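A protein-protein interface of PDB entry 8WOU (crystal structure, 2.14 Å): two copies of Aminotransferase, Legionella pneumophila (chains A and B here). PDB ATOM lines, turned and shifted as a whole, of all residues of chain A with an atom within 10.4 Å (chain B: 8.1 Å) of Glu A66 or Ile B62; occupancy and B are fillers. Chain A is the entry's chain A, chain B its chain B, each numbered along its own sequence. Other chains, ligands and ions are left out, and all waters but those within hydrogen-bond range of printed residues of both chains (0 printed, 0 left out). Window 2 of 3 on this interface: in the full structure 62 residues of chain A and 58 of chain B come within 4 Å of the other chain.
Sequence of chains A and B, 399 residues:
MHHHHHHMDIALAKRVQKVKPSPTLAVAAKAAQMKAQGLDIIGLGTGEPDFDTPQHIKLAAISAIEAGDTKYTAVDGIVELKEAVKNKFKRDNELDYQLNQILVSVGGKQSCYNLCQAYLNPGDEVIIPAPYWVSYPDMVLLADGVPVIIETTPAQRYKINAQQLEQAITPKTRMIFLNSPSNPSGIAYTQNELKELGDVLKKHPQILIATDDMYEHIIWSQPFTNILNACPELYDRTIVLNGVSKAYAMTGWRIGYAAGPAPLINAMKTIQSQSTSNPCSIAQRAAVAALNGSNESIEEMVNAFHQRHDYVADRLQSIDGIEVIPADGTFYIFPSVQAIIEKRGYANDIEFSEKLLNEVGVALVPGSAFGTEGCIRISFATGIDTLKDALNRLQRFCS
The side-chain carboxylate (OD1) of Asp B52 lies within hydrogen-bond range of the side-chain hydroxyl (OG1) of Thr A70 (3.4 Å). The side-chain amino group of Lys A58 is in hydrogen-bond range of the backbone carbonyl oxygen of Ile B65 (3.3 Å). The side-chain amino group of Lys B58 is in hydrogen-bond range of the backbone carbonyl oxygen of Ile A65 (2.8 Å).
NZ of Lys B58 lies within salt-bridge range of OD1 of Asp B52 (3.2 Å). The side-chain carboxylate (OD2) of Asp A52 lies within salt-bridge range of the side-chain amino group (NZ) of Lys A58 (2.4 Å).
Gly B68 touches Asp A52. Ala A61 touches Ile B65 (CB to CD1, 3.98 Å). Ile A62 touches Ile B62. Ile A62 touches Ile B65 (CG1 to CD1, 3.8 Å). Ile A62 touches Glu B66. Ala B61 touches Ile A65 (CB to CD1, 3.9 Å). Ile B62 touches Ile A65. Ile A65 touches Trp B253 (CG1 to CH2, 3.7 Å). CA of Gly A68 touches OD1 of Asp B52 (3.6 Å). N of Gly A68 touches NZ of Lys B58, 3.8 Å away.
Of the printed residues of chain B, Lys A58 touches Ile B65 (3.3 Å). Of the printed residues of chain B, Ala A61 touches Ile B65. Of the printed residues of chain B, Glu A66 touches Ile B62 (3.8 Å). Ala A67 touches none of the printed residues of chain B. Printed residues of chain B within 4 Å of Thr A70: Asp B52 (3.4 Å) and Trp B253 (3.3 Å). Ala B60 touches none of the printed residues of chain A. Ala B61 touches just one residue of chain A: Ile A65 (3.9 Å). No residue of chain A comes within 4 Å of Ser B63. No residue of chain A comes within 4 Å of Ala B64. Of the printed residues of chain A, Ile B65 touches Lys A58 (3.3 Å), Ala A61 (3.98 Å), Ile A62 (3.8 Å) and Ile A65 (3.9 Å). Glu B66 touches just one residue of chain A: Ile A62 (3.9 Å). Of the printed residues of chain A, Trp B253 touches Ile A65 (3.7 Å) and Thr A70 (3.3 Å). Arg B285 touches none of the printed residues of chain A. The nearest printed residue of chain B that does not touch Glu A66 is Lys B58 (4.01 Å). The nearest residue of chain A that does not touch Ile B62 is Ala A61 (6.2 Å). The nearest printed residue of chain B that does not touch Ile A65 is Ile B282 (4.9 Å).
Printed residues of chain A that touch a printed residue of chain B: Asp A52, Lys A58, Ala A61, Ile A62, Ile A65, Glu A66, Gly A68 and Thr A70. Hydrophobic or aromatic side chains of chain A that line the printed part of chain B: Ala A61, Ile A62 and Ile A65. Along chain B the printed residues that touch a printed residue of chain A span positions 52 to 253. Among the printed residues, no Asp or Glu carboxylate lies within 4 Å of a Lys or Arg side-chain nitrogen of the other chain.
Asp A52 touches Gly B68, and with the chains exchanged Gly A68 touches Asp B52. Ala A61 touches Ile B65, and with the chains exchanged Ile A65 touches Ala B61. Ile A62 touches Ile B65, and with the chains exchanged Ile A65 touches Ile B62. Gly A68 touches Lys B58, but with the chains exchanged Lys A58 does not touch Gly B68 (4.4 Å). Of the 16 pairs that touch across the chains among the printed residues, 12 have their exchanged pair printed and touching as well.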
ATOM      1  N   ASP A  52     -27.835   3.899  21.014  1.00  0.00           N
ATOM      2  CA  ASP A  52     -27.387   3.286  19.780  1.00  0.00           C
ATOM      3  C   ASP A  52     -27.435   1.772  19.919  1.00  0.00           C
ATOM      4  O   ASP A  52     -27.455   1.224  21.026  1.00  0.00           O
ATOM      5  CB  ASP A  52     -25.978   3.740  19.404  1.00  0.00           C
ATOM      6  CG  ASP A  52     -25.704   3.597  17.913  1.00  0.00           C
ATOM      7  OD1 ASP A  52     -26.642   3.245  17.163  1.00  0.00           O
ATOM      8  OD2 ASP A  52     -24.554   3.837  17.489  1.00  0.00           O
ATOM      9  N   GLN A  55     -22.691  -2.417  20.912  1.00  0.00           N
ATOM     10  CA  GLN A  55     -21.521  -2.566  20.052  1.00  0.00           C
ATOM     11  C   GLN A  55     -21.388  -3.985  19.498  1.00  0.00           C
ATOM     12  O   GLN A  55     -20.967  -4.160  18.351  1.00  0.00           O
ATOM     13  CB  GLN A  55     -20.248  -2.144  20.796  1.00  0.00           C
ATOM     14  CG  GLN A  55     -18.997  -1.998  19.890  1.00  0.00           C
ATOM     15  CD  GLN A  55     -19.240  -1.135  18.638  1.00  0.00           C
ATOM     16  OE1 GLN A  55     -19.119  -1.615  17.505  1.00  0.00           O
ATOM     17  NE2 GLN A  55     -19.570   0.140  18.844  1.00  0.00           N
ATOM     18  N   ILE A  57     -23.708  -6.055  18.612  1.00  0.00           N
ATOM     19  CA  ILE A  57     -24.597  -6.207  17.463  1.00  0.00           C
ATOM     20  C   ILE A  57     -23.988  -5.555  16.226  1.00  0.00           C
ATOM     21  O   ILE A  57     -24.048  -6.107  15.120  1.00  0.00           O
ATOM     22  CB  ILE A  57     -25.990  -5.649  17.794  1.00  0.00           C
ATOM     23  CG1 ILE A  57     -26.639  -6.515  18.872  1.00  0.00           C
ATOM     24  CG2 ILE A  57     -26.853  -5.608  16.565  1.00  0.00           C
ATOM     25  CD1 ILE A  57     -27.849  -5.853  19.520  1.00  0.00           C
ATOM     26  N   LYS A  58     -23.338  -4.409  16.397  1.00  0.00           N
ATOM     27  CA  LYS A  58     -22.734  -3.739  15.250  1.00  0.00           C
ATOM     28  C   LYS A  58     -21.608  -4.577  14.662  1.00  0.00           C
ATOM     29  O   LYS A  58     -21.527  -4.771  13.436  1.00  0.00           O
ATOM     30  CB  LYS A  58     -22.219  -2.361  15.665  1.00  0.00           C
ATOM     31  CG  LYS A  58     -23.279  -1.492  16.309  1.00  0.00           C
ATOM     32  CD  LYS A  58     -23.288  -0.096  15.712  1.00  0.00           C
ATOM     33  CE  LYS A  58     -22.539   0.889  16.589  1.00  0.00           C
ATOM     34  NZ  LYS A  58     -23.086   2.264  16.417  1.00  0.00           N
ATOM     35  N   LEU A  59     -20.725  -5.084  15.530  1.00  0.00           N
ATOM     36  CA  LEU A  59     -19.602  -5.882  15.060  1.00  0.00           C
ATOM     37  C   LEU A  59     -20.071  -7.119  14.321  1.00  0.00           C
ATOM     38  O   LEU A  59     -19.403  -7.575  13.390  1.00  0.00           O
ATOM     39  CB  LEU A  59     -18.709  -6.270  16.239  1.00  0.00           C
ATOM     40  CG  LEU A  59     -18.229  -5.033  17.001  1.00  0.00           C
ATOM     41  CD1 LEU A  59     -17.282  -5.368  18.164  1.00  0.00           C
ATOM     42  CD2 LEU A  59     -17.585  -4.048  16.030  1.00  0.00           C
ATOM     43  N   ALA A  60     -21.219  -7.674  14.703  1.00  0.00           N
ATOM     44  CA  ALA A  60     -21.690  -8.868  14.007  1.00  0.00           C
ATOM     45  C   ALA A  60     -22.209  -8.515  12.623  1.00  0.00           C
ATOM     46  O   ALA A  60     -22.048  -9.287  11.671  1.00  0.00           O
ATOM     47  CB  ALA A  60     -22.770  -9.566  14.828  1.00  0.00           C
ATOM     48  N   ALA A  61     -22.846  -7.352  12.499  1.00  0.00           N
ATOM     49  CA  ALA A  61     -23.323  -6.916  11.195  1.00  0.00           C
ATOM     50  C   ALA A  61     -22.153  -6.554  10.285  1.00  0.00           C
ATOM     51  O   ALA A  61     -22.133  -6.935   9.111  1.00  0.00           O
ATOM     52  CB  ALA A  61     -24.272  -5.737  11.360  1.00  0.00           C
ATOM     53  N   ILE A  62     -21.166  -5.832  10.822  1.00  0.00           N
ATOM     54  CA  ILE A  62     -19.944  -5.523  10.080  1.00  0.00           C
ATOM     55  C   ILE A  62     -19.246  -6.806   9.652  1.00  0.00           C
ATOM     56  O   ILE A  62     -18.907  -6.997   8.477  1.00  0.00           O
ATOM     57  CB  ILE A  62     -18.998  -4.661  10.934  1.00  0.00           C
ATOM     58  CG1 ILE A  62     -19.534  -3.236  11.065  1.00  0.00           C
ATOM     59  CG2 ILE A  62     -17.588  -4.688  10.350  1.00  0.00           C
ATOM     60  CD1 ILE A  62     -18.619  -2.328  11.867  1.00  0.00           C
ATOM     61  N   SER A  63     -18.986  -7.685  10.620  1.00  0.00           N
ATOM     62  CA  SER A  63     -18.327  -8.941  10.319  1.00  0.00           C
ATOM     63  C   SER A  63     -19.107  -9.731   9.280  1.00  0.00           C
ATOM     64  O   SER A  63     -18.517 -10.385   8.417  1.00  0.00           O
ATOM     65  CB  SER A  63     -18.153  -9.754  11.595  1.00  0.00           C
ATOM     66  OG  SER A  63     -18.025 -11.118  11.276  1.00  0.00           O
ATOM     67  N   ALA A  64     -20.438  -9.664   9.328  1.00  0.00           N
ATOM     68  CA  ALA A  64     -21.238 -10.343   8.314  1.00  0.00           C
ATOM     69  C   ALA A  64     -21.035  -9.732   6.928  1.00  0.00           C
ATOM     70  O   ALA A  64     -21.061 -10.450   5.922  1.00  0.00           O
ATOM     71  CB  ALA A  64     -22.713 -10.303   8.703  1.00  0.00           C
ATOM     72  N   ILE A  65     -20.861  -8.406   6.854  1.00  0.00           N
ATOM     73  CA  ILE A  65     -20.638  -7.736   5.572  1.00  0.00           C
ATOM     74  C   ILE A  65     -19.303  -8.151   4.982  1.00  0.00           C
ATOM     75  O   ILE A  65     -19.157  -8.279   3.763  1.00  0.00           O
ATOM     76  CB  ILE A  65     -20.717  -6.205   5.762  1.00  0.00           C
ATOM     77  CG1 ILE A  65     -22.157  -5.729   5.674  1.00  0.00           C
ATOM     78  CG2 ILE A  65     -19.881  -5.452   4.741  1.00  0.00           C
ATOM     79  CD1 ILE A  65     -22.333  -4.317   6.236  1.00  0.00           C
ATOM     80  N   GLU A  66     -18.307  -8.385   5.838  1.00  0.00           N
ATOM     81  CA  GLU A  66     -16.989  -8.765   5.355  1.00  0.00           C
ATOM     82  C   GLU A  66     -16.928 -10.211   4.898  1.00  0.00           C
ATOM     83  O   GLU A  66     -16.056 -10.557   4.100  1.00  0.00           O
ATOM     84  CB  GLU A  66     -15.953  -8.515   6.445  1.00  0.00           C
ATOM     85  CG  GLU A  66     -15.791  -7.045   6.759  1.00  0.00           C
ATOM     86  CD  GLU A  66     -14.849  -6.803   7.902  1.00  0.00           C
ATOM     87  OE1 GLU A  66     -14.597  -5.622   8.218  1.00  0.00           O
ATOM     88  OE2 GLU A  66     -14.367  -7.798   8.488  1.00  0.00           O
ATOM     89  N   ALA A  67     -17.843 -11.053   5.363  1.00  0.00           N
ATOM     90  CA  ALA A  67     -17.804 -12.464   5.005  1.00  0.00           C
ATOM     91  C   ALA A  67     -18.446 -12.753   3.656  1.00  0.00           C
ATOM     92  O   ALA A  67     -18.252 -13.849   3.119  1.00  0.00           O
ATOM     93  CB  ALA A  67     -18.491 -13.291   6.092  1.00  0.00           C
ATOM     94  N   GLY A  68     -19.197 -11.807   3.098  1.00  0.00           N
ATOM     95  CA  GLY A  68     -19.938 -12.069   1.882  1.00  0.00           C
ATOM     96  C   GLY A  68     -21.372 -12.495   2.106  1.00  0.00           C
ATOM     97  O   GLY A  68     -21.959 -13.148   1.232  1.00  0.00           O
ATOM     98  N   ASP A  69     -21.953 -12.156   3.259  1.00  0.00           N
ATOM     99  CA  ASP A  69     -23.355 -12.455   3.577  1.00  0.00           C
ATOM    100  C   ASP A  69     -24.334 -11.519   2.871  1.00  0.00           C
ATOM    101  O   ASP A  69     -25.312 -11.060   3.469  1.00  0.00           O
ATOM    102  CB  ASP A  69     -23.552 -12.399   5.092  1.00  0.00           C
ATOM    103  CG  ASP A  69     -23.242 -13.726   5.781  1.00  0.00           C
ATOM    104  OD1 ASP A  69     -23.327 -14.784   5.117  1.00  0.00           O
ATOM    105  OD2 ASP A  69     -22.905 -13.711   6.986  1.00  0.00           O
ATOM    106  N   THR A  70     -24.102 -11.248   1.585  1.00  0.00           N
ATOM    107  CA  THR A  70     -24.822 -10.228   0.834  1.00  0.00           C
ATOM    108  C   THR A  70     -25.781 -10.832  -0.191  1.00  0.00           C
ATOM    109  O   THR A  70     -26.091 -10.202  -1.209  1.00  0.00           O
ATOM    110  CB  THR A  70     -23.822  -9.300   0.145  1.00  0.00           C
ATOM    111  OG1 THR A  70     -22.899 -10.081  -0.630  1.00  0.00           O
ATOM    112  CG2 THR A  70     -23.043  -8.515   1.171  1.00  0.00           C
ATOM    113  N   TRP A 253     -33.100  -1.231  11.529  1.00  0.00           N
ATOM    114  CA  TRP A 253     -32.622  -2.472  10.914  1.00  0.00           C
ATOM    115  C   TRP A 253     -33.728  -3.303  10.267  1.00  0.00           C
ATOM    116  O   TRP A 253     -33.430  -4.131   9.401  1.00  0.00           O
ATOM    117  CB  TRP A 253     -31.901  -3.338  11.940  1.00  0.00           C
ATOM    118  CG  TRP A 253     -30.666  -2.734  12.481  1.00  0.00           C
ATOM    119  CD1 TRP A 253     -30.574  -1.846  13.503  1.00  0.00           C
ATOM    120  CD2 TRP A 253     -29.318  -3.004  12.062  1.00  0.00           C
ATOM    121  NE1 TRP A 253     -29.257  -1.535  13.752  1.00  0.00           N
ATOM    122  CE2 TRP A 253     -28.465  -2.234  12.879  1.00  0.00           C
ATOM    123  CE3 TRP A 253     -28.757  -3.813  11.083  1.00  0.00           C
ATOM    124  CZ2 TRP A 253     -27.082  -2.247  12.738  1.00  0.00           C
ATOM    125  CZ3 TRP A 253     -27.376  -3.822  10.940  1.00  0.00           C
ATOM    126  CH2 TRP A 253     -26.556  -3.046  11.765  1.00  0.00           C
ATOM    127  N   SER A 281     -29.996  -9.516   4.631  1.00  0.00           N
ATOM    128  CA  SER A 281     -29.226 -10.594   5.239  1.00  0.00           C
ATOM    129  C   SER A 281     -28.228 -10.081   6.267  1.00  0.00           C
ATOM    130  O   SER A 281     -27.928 -10.779   7.246  1.00  0.00           O
ATOM    131  CB  SER A 281     -28.499 -11.398   4.160  1.00  0.00           C
ATOM    132  OG  SER A 281     -27.910 -10.528   3.211  1.00  0.00           O
ATOM    133  N   ILE A 282     -27.690  -8.876   6.073  1.00  0.00           N
ATOM    134  CA  ILE A 282     -26.821  -8.307   7.099  1.00  0.00           C
ATOM    135  C   ILE A 282     -27.612  -8.046   8.377  1.00  0.00           C
ATOM    136  O   ILE A 282     -27.099  -8.206   9.495  1.00  0.00           O
ATOM    137  CB  ILE A 282     -26.148  -7.022   6.581  1.00  0.00           C
ATOM    138  CG1 ILE A 282     -25.399  -7.297   5.264  1.00  0.00           C
ATOM    139  CG2 ILE A 282     -25.241  -6.426   7.665  1.00  0.00           C
ATOM    140  CD1 ILE A 282     -24.611  -8.660   5.216  1.00  0.00           C
ATOM    141  N   ARG A 285     -28.143 -11.260  10.414  1.00  0.00           N
ATOM    142  CA  ARG A 285     -26.958 -11.547  11.207  1.00  0.00           C
ATOM    143  C   ARG A 285     -26.892 -10.672  12.455  1.00  0.00           C
ATOM    144  O   ARG A 285     -26.582 -11.154  13.552  1.00  0.00           O
ATOM    145  CB  ARG A 285     -25.710 -11.356  10.350  1.00  0.00           C
ATOM    146  CG  ARG A 285     -25.576 -12.387   9.264  1.00  0.00           C
ATOM    147  CD  ARG A 285     -25.462 -13.802   9.836  1.00  0.00           C
ATOM    148  NE  ARG A 285     -25.341 -14.791   8.767  1.00  0.00           N
ATOM    149  CZ  ARG A 285     -25.146 -16.097   8.957  1.00  0.00           C
ATOM    150  NH1 ARG A 285     -25.046 -16.602  10.187  1.00  0.00           N
ATOM    151  NH2 ARG A 285     -25.046 -16.900   7.906  1.00  0.00           N
ATOM    152  N   ASP B  52     -19.097 -10.863  -5.242  1.00  0.00           N
ATOM    153  CA  ASP B  52     -19.379 -10.180  -3.993  1.00  0.00           C
ATOM    154  C   ASP B  52     -19.869  -8.754  -4.256  1.00  0.00           C
ATOM    155  O   ASP B  52     -19.738  -8.200  -5.354  1.00  0.00           O
ATOM    156  CB  ASP B  52     -18.145 -10.162  -3.090  1.00  0.00           C
ATOM    157  CG  ASP B  52     -18.471 -10.591  -1.664  1.00  0.00           C
ATOM    158  OD1 ASP B  52     -19.573 -10.233  -1.178  1.00  0.00           O
ATOM    159  OD2 ASP B  52     -17.640 -11.297  -1.045  1.00  0.00           O
ATOM    160  N   GLN B  55     -16.139  -3.480  -3.016  1.00  0.00           N
ATOM    161  CA  GLN B  55     -15.545  -3.031  -1.768  1.00  0.00           C
ATOM    162  C   GLN B  55     -16.011  -1.637  -1.388  1.00  0.00           C
ATOM    163  O   GLN B  55     -16.267  -1.373  -0.210  1.00  0.00           O
ATOM    164  CB  GLN B  55     -14.021  -3.079  -1.862  1.00  0.00           C
ATOM    165  CG  GLN B  55     -13.341  -3.066  -0.508  1.00  0.00           C
ATOM    166  CD  GLN B  55     -13.792  -4.219   0.373  1.00  0.00           C
ATOM    167  OE1 GLN B  55     -14.058  -5.318  -0.116  1.00  0.00           O
ATOM    168  NE2 GLN B  55     -13.881  -3.975   1.677  1.00  0.00           N
ATOM    169  N   HIS B  56     -16.126  -0.722  -2.358  1.00  0.00           N
ATOM    170  CA  HIS B  56     -16.491   0.640  -1.982  1.00  0.00           C
ATOM    171  C   HIS B  56     -17.908   0.702  -1.419  1.00  0.00           C
ATOM    172  O   HIS B  56     -18.182   1.510  -0.521  1.00  0.00           O
ATOM    173  CB  HIS B  56     -16.297   1.599  -3.163  1.00  0.00           C
ATOM    174  CG  HIS B  56     -17.278   1.428  -4.285  1.00  0.00           C
ATOM    175  ND1 HIS B  56     -17.129   0.468  -5.265  1.00  0.00           N
ATOM    176  CD2 HIS B  56     -18.393   2.129  -4.613  1.00  0.00           C
ATOM    177  CE1 HIS B  56     -18.119   0.571  -6.135  1.00  0.00           C
ATOM    178  NE2 HIS B  56     -18.896   1.576  -5.768  1.00  0.00           N
ATOM    179  N   ILE B  57     -18.800  -0.171  -1.886  1.00  0.00           N
ATOM    180  CA  ILE B  57     -20.139  -0.252  -1.305  1.00  0.00           C
ATOM    181  C   ILE B  57     -20.064  -0.819   0.108  1.00  0.00           C
ATOM    182  O   ILE B  57     -20.651  -0.271   1.046  1.00  0.00           O
ATOM    183  CB  ILE B  57     -21.058  -1.089  -2.209  1.00  0.00           C
ATOM    184  CG1 ILE B  57     -21.185  -0.417  -3.572  1.00  0.00           C
ATOM    185  CG2 ILE B  57     -22.436  -1.281  -1.572  1.00  0.00           C
ATOM    186  CD1 ILE B  57     -21.459  -1.380  -4.726  1.00  0.00           C
ATOM    187  N   LYS B  58     -19.320  -1.915   0.281  1.00  0.00           N
ATOM    188  CA  LYS B  58     -19.182  -2.529   1.598  1.00  0.00           C
ATOM    189  C   LYS B  58     -18.611  -1.542   2.605  1.00  0.00           C
ATOM    190  O   LYS B  58     -19.111  -1.424   3.729  1.00  0.00           O
ATOM    191  CB  LYS B  58     -18.289  -3.766   1.514  1.00  0.00           C
ATOM    192  CG  LYS B  58     -18.937  -4.960   0.853  1.00  0.00           C
ATOM    193  CD  LYS B  58     -18.055  -6.199   1.005  1.00  0.00           C
ATOM    194  CE  LYS B  58     -18.854  -7.465   0.765  1.00  0.00           C
ATOM    195  NZ  LYS B  58     -18.128  -8.680   1.221  1.00  0.00           N
ATOM    196  N   LEU B  59     -17.545  -0.836   2.220  1.00  0.00           N
ATOM    197  CA  LEU B  59     -16.948   0.150   3.112  1.00  0.00           C
ATOM    198  C   LEU B  59     -17.963   1.199   3.528  1.00  0.00           C
ATOM    199  O   LEU B  59     -18.046   1.557   4.709  1.00  0.00           O
ATOM    200  CB  LEU B  59     -15.745   0.814   2.445  1.00  0.00           C
ATOM    201  CG  LEU B  59     -14.598  -0.148   2.108  1.00  0.00           C
ATOM    202  CD1 LEU B  59     -13.595   0.480   1.127  1.00  0.00           C
ATOM    203  CD2 LEU B  59     -13.913  -0.629   3.378  1.00  0.00           C
ATOM    204  N   ALA B  60     -18.749   1.697   2.568  1.00  0.00           N
ATOM    205  CA  ALA B  60     -19.739   2.722   2.879  1.00  0.00           C
ATOM    206  C   ALA B  60     -20.765   2.213   3.880  1.00  0.00           C
ATOM    207  O   ALA B  60     -21.186   2.958   4.772  1.00  0.00           O
ATOM    208  CB  ALA B  60     -20.435   3.192   1.605  1.00  0.00           C
ATOM    209  N   ALA B  61     -21.178   0.948   3.752  1.00  0.00           N
ATOM    210  CA  ALA B  61     -22.139   0.379   4.696  1.00  0.00           C
ATOM    211  C   ALA B  61     -21.529   0.236   6.085  1.00  0.00           C
ATOM    212  O   ALA B  61     -22.157   0.593   7.086  1.00  0.00           O
ATOM    213  CB  ALA B  61     -22.641  -0.974   4.196  1.00  0.00           C
ATOM    214  N   ILE B  62     -20.306  -0.296   6.163  1.00  0.00           N
ATOM    215  CA  ILE B  62     -19.621  -0.438   7.448  1.00  0.00           C
ATOM    216  C   ILE B  62     -19.546   0.915   8.153  1.00  0.00           C
ATOM    217  O   ILE B  62     -19.888   1.047   9.338  1.00  0.00           O
ATOM    218  CB  ILE B  62     -18.225  -1.061   7.240  1.00  0.00           C
ATOM    219  CG1 ILE B  62     -18.351  -2.545   6.866  1.00  0.00           C
ATOM    220  CG2 ILE B  62     -17.360  -0.880   8.485  1.00  0.00           C
ATOM    221  CD1 ILE B  62     -17.054  -3.224   6.483  1.00  0.00           C
ATOM    222  N   SER B  63     -19.148   1.951   7.409  1.00  0.00           N
ATOM    223  CA  SER B  63     -19.041   3.287   7.980  1.00  0.00           C
ATOM    224  C   SER B  63     -20.394   3.827   8.439  1.00  0.00           C
ATOM    225  O   SER B  63     -20.461   4.610   9.392  1.00  0.00           O
ATOM    226  CB  SER B  63     -18.401   4.223   6.959  1.00  0.00           C
ATOM    227  OG  SER B  63     -18.848   5.549   7.143  1.00  0.00           O
ATOM    228  N   ALA B  64     -21.485   3.421   7.795  1.00  0.00           N
ATOM    229  CA  ALA B  64     -22.782   3.875   8.275  1.00  0.00           C
ATOM    230  C   ALA B  64     -23.190   3.153   9.553  1.00  0.00           C
ATOM    231  O   ALA B  64     -23.932   3.713  10.367  1.00  0.00           O
ATOM    232  CB  ALA B  64     -23.844   3.689   7.195  1.00  0.00           C
ATOM    233  N   ILE B  65     -22.733   1.912   9.740  1.00  0.00           N
ATOM    234  CA  ILE B  65     -22.977   1.206  10.996  1.00  0.00           C
ATOM    235  C   ILE B  65     -22.271   1.917  12.141  1.00  0.00           C
ATOM    236  O   ILE B  65     -22.892   2.285  13.146  1.00  0.00           O
ATOM    237  CB  ILE B  65     -22.525  -0.263  10.889  1.00  0.00           C
ATOM    238  CG1 ILE B  65     -23.515  -1.065  10.055  1.00  0.00           C
ATOM    239  CG2 ILE B  65     -22.409  -0.863  12.263  1.00  0.00           C
ATOM    240  CD1 ILE B  65     -22.985  -2.401   9.605  1.00  0.00           C
ATOM    241  N   GLU B  66     -20.962   2.139  11.992  1.00  0.00           N
ATOM    242  CA  GLU B  66     -20.191   2.829  13.020  1.00  0.00           C
ATOM    243  C   GLU B  66     -20.679   4.250  13.273  1.00  0.00           C
ATOM    244  O   GLU B  66     -20.428   4.793  14.352  1.00  0.00           O
ATOM    245  CB  GLU B  66     -18.715   2.852  12.628  1.00  0.00           C
ATOM    246  CG  GLU B  66     -18.266   1.572  11.955  1.00  0.00           C
ATOM    247  CD  GLU B  66     -16.772   1.535  11.690  1.00  0.00           C
ATOM    248  OE1 GLU B  66     -16.093   0.658  12.262  1.00  0.00           O
ATOM    249  OE2 GLU B  66     -16.277   2.382  10.910  1.00  0.00           O
ATOM    250  N   ALA B  67     -21.374   4.865  12.320  1.00  0.00           N
ATOM    251  CA  ALA B  67     -21.827   6.237  12.495  1.00  0.00           C
ATOM    252  C   ALA B  67     -23.229   6.346  13.092  1.00  0.00           C
ATOM    253  O   ALA B  67     -23.686   7.467  13.353  1.00  0.00           O
ATOM    254  CB  ALA B  67     -21.785   6.986  11.159  1.00  0.00           C
ATOM    255  N   GLY B  68     -23.923   5.228  13.295  1.00  0.00           N
ATOM    256  CA  GLY B  68     -25.195   5.255  13.991  1.00  0.00           C
ATOM    257  C   GLY B  68     -26.406   5.622  13.162  1.00  0.00           C
ATOM    258  O   GLY B  68     -27.431   6.019  13.731  1.00  0.00           O
ATOM    259  N   TRP B 253     -29.112  -7.247  -0.053  1.00  0.00           N
ATOM    260  CA  TRP B 253     -29.268  -5.947   0.590  1.00  0.00           C
ATOM    261  C   TRP B 253     -30.705  -5.430   0.566  1.00  0.00           C
ATOM    262  O   TRP B 253     -31.075  -4.634   1.432  1.00  0.00           O
ATOM    263  CB  TRP B 253     -28.336  -4.942  -0.070  1.00  0.00           C
ATOM    264  CG  TRP B 253     -26.891  -5.216   0.170  1.00  0.00           C
ATOM    265  CD1 TRP B 253     -26.057  -5.996  -0.588  1.00  0.00           C
ATOM    266  CD2 TRP B 253     -26.096  -4.707   1.247  1.00  0.00           C
ATOM    267  NE1 TRP B 253     -24.792  -5.992  -0.050  1.00  0.00           N
ATOM    268  CE2 TRP B 253     -24.792  -5.213   1.080  1.00  0.00           C
ATOM    269  CE3 TRP B 253     -26.363  -3.868   2.331  1.00  0.00           C
ATOM    270  CZ2 TRP B 253     -23.752  -4.901   1.956  1.00  0.00           C
ATOM    271  CZ3 TRP B 253     -25.343  -3.574   3.199  1.00  0.00           C
ATOM    272  CH2 TRP B 253     -24.047  -4.086   3.007  1.00  0.00           C
ATOM    273  N   ILE B 282     -29.019   1.121   6.680  1.00  0.00           N
ATOM    274  CA  ILE B 282     -27.663   0.745   6.268  1.00  0.00           C
ATOM    275  C   ILE B 282     -27.622   0.427   4.777  1.00  0.00           C
ATOM    276  O   ILE B 282     -26.711   0.856   4.056  1.00  0.00           O
ATOM    277  CB  ILE B 282     -27.160  -0.446   7.108  1.00  0.00           C
ATOM    278  CG1 ILE B 282     -27.320  -0.152   8.598  1.00  0.00           C
ATOM    279  CG2 ILE B 282     -25.709  -0.760   6.792  1.00  0.00           C
ATOM    280  CD1 ILE B 282     -26.597   1.110   9.028  1.00  0.00           C
ATOM    281  N   ARG B 285     -27.550   3.570   2.501  1.00  0.00           N
ATOM    282  CA  ARG B 285     -26.234   4.183   2.345  1.00  0.00           C
ATOM    283  C   ARG B 285     -25.356   3.374   1.404  1.00  0.00           C
ATOM    284  O   ARG B 285     -24.630   3.944   0.578  1.00  0.00           O
ATOM    285  CB  ARG B 285     -25.541   4.314   3.695  1.00  0.00           C
ATOM    286  CG  ARG B 285     -26.296   5.145   4.670  1.00  0.00           C
ATOM    287  CD  ARG B 285     -26.006   6.603   4.488  1.00  0.00           C
ATOM    288  NE  ARG B 285     -26.974   7.387   5.247  1.00  0.00           N
ATOM    289  CZ  ARG B 285     -27.006   8.713   5.279  1.00  0.00           C
ATOM    290  NH1 ARG B 285     -26.114   9.417   4.590  1.00  0.00           N
ATOM    291  NH2 ARG B 285     -27.935   9.334   5.996  1.00  0.00           N
ATOM    292  N   ALA B 286     -25.386   2.046   1.540  1.00  0.00           N
ATOM    293  CA  ALA B 286     -24.694   1.196   0.580  1.00  0.00           C
ATOM    294  C   ALA B 286     -25.202   1.445  -0.834  1.00  0.00           C
ATOM    295  O   ALA B 286     -24.415   1.479  -1.788  1.00  0.00           O
ATOM    296  CB  ALA B 286     -24.853  -0.279   0.963  1.00  0.00           C
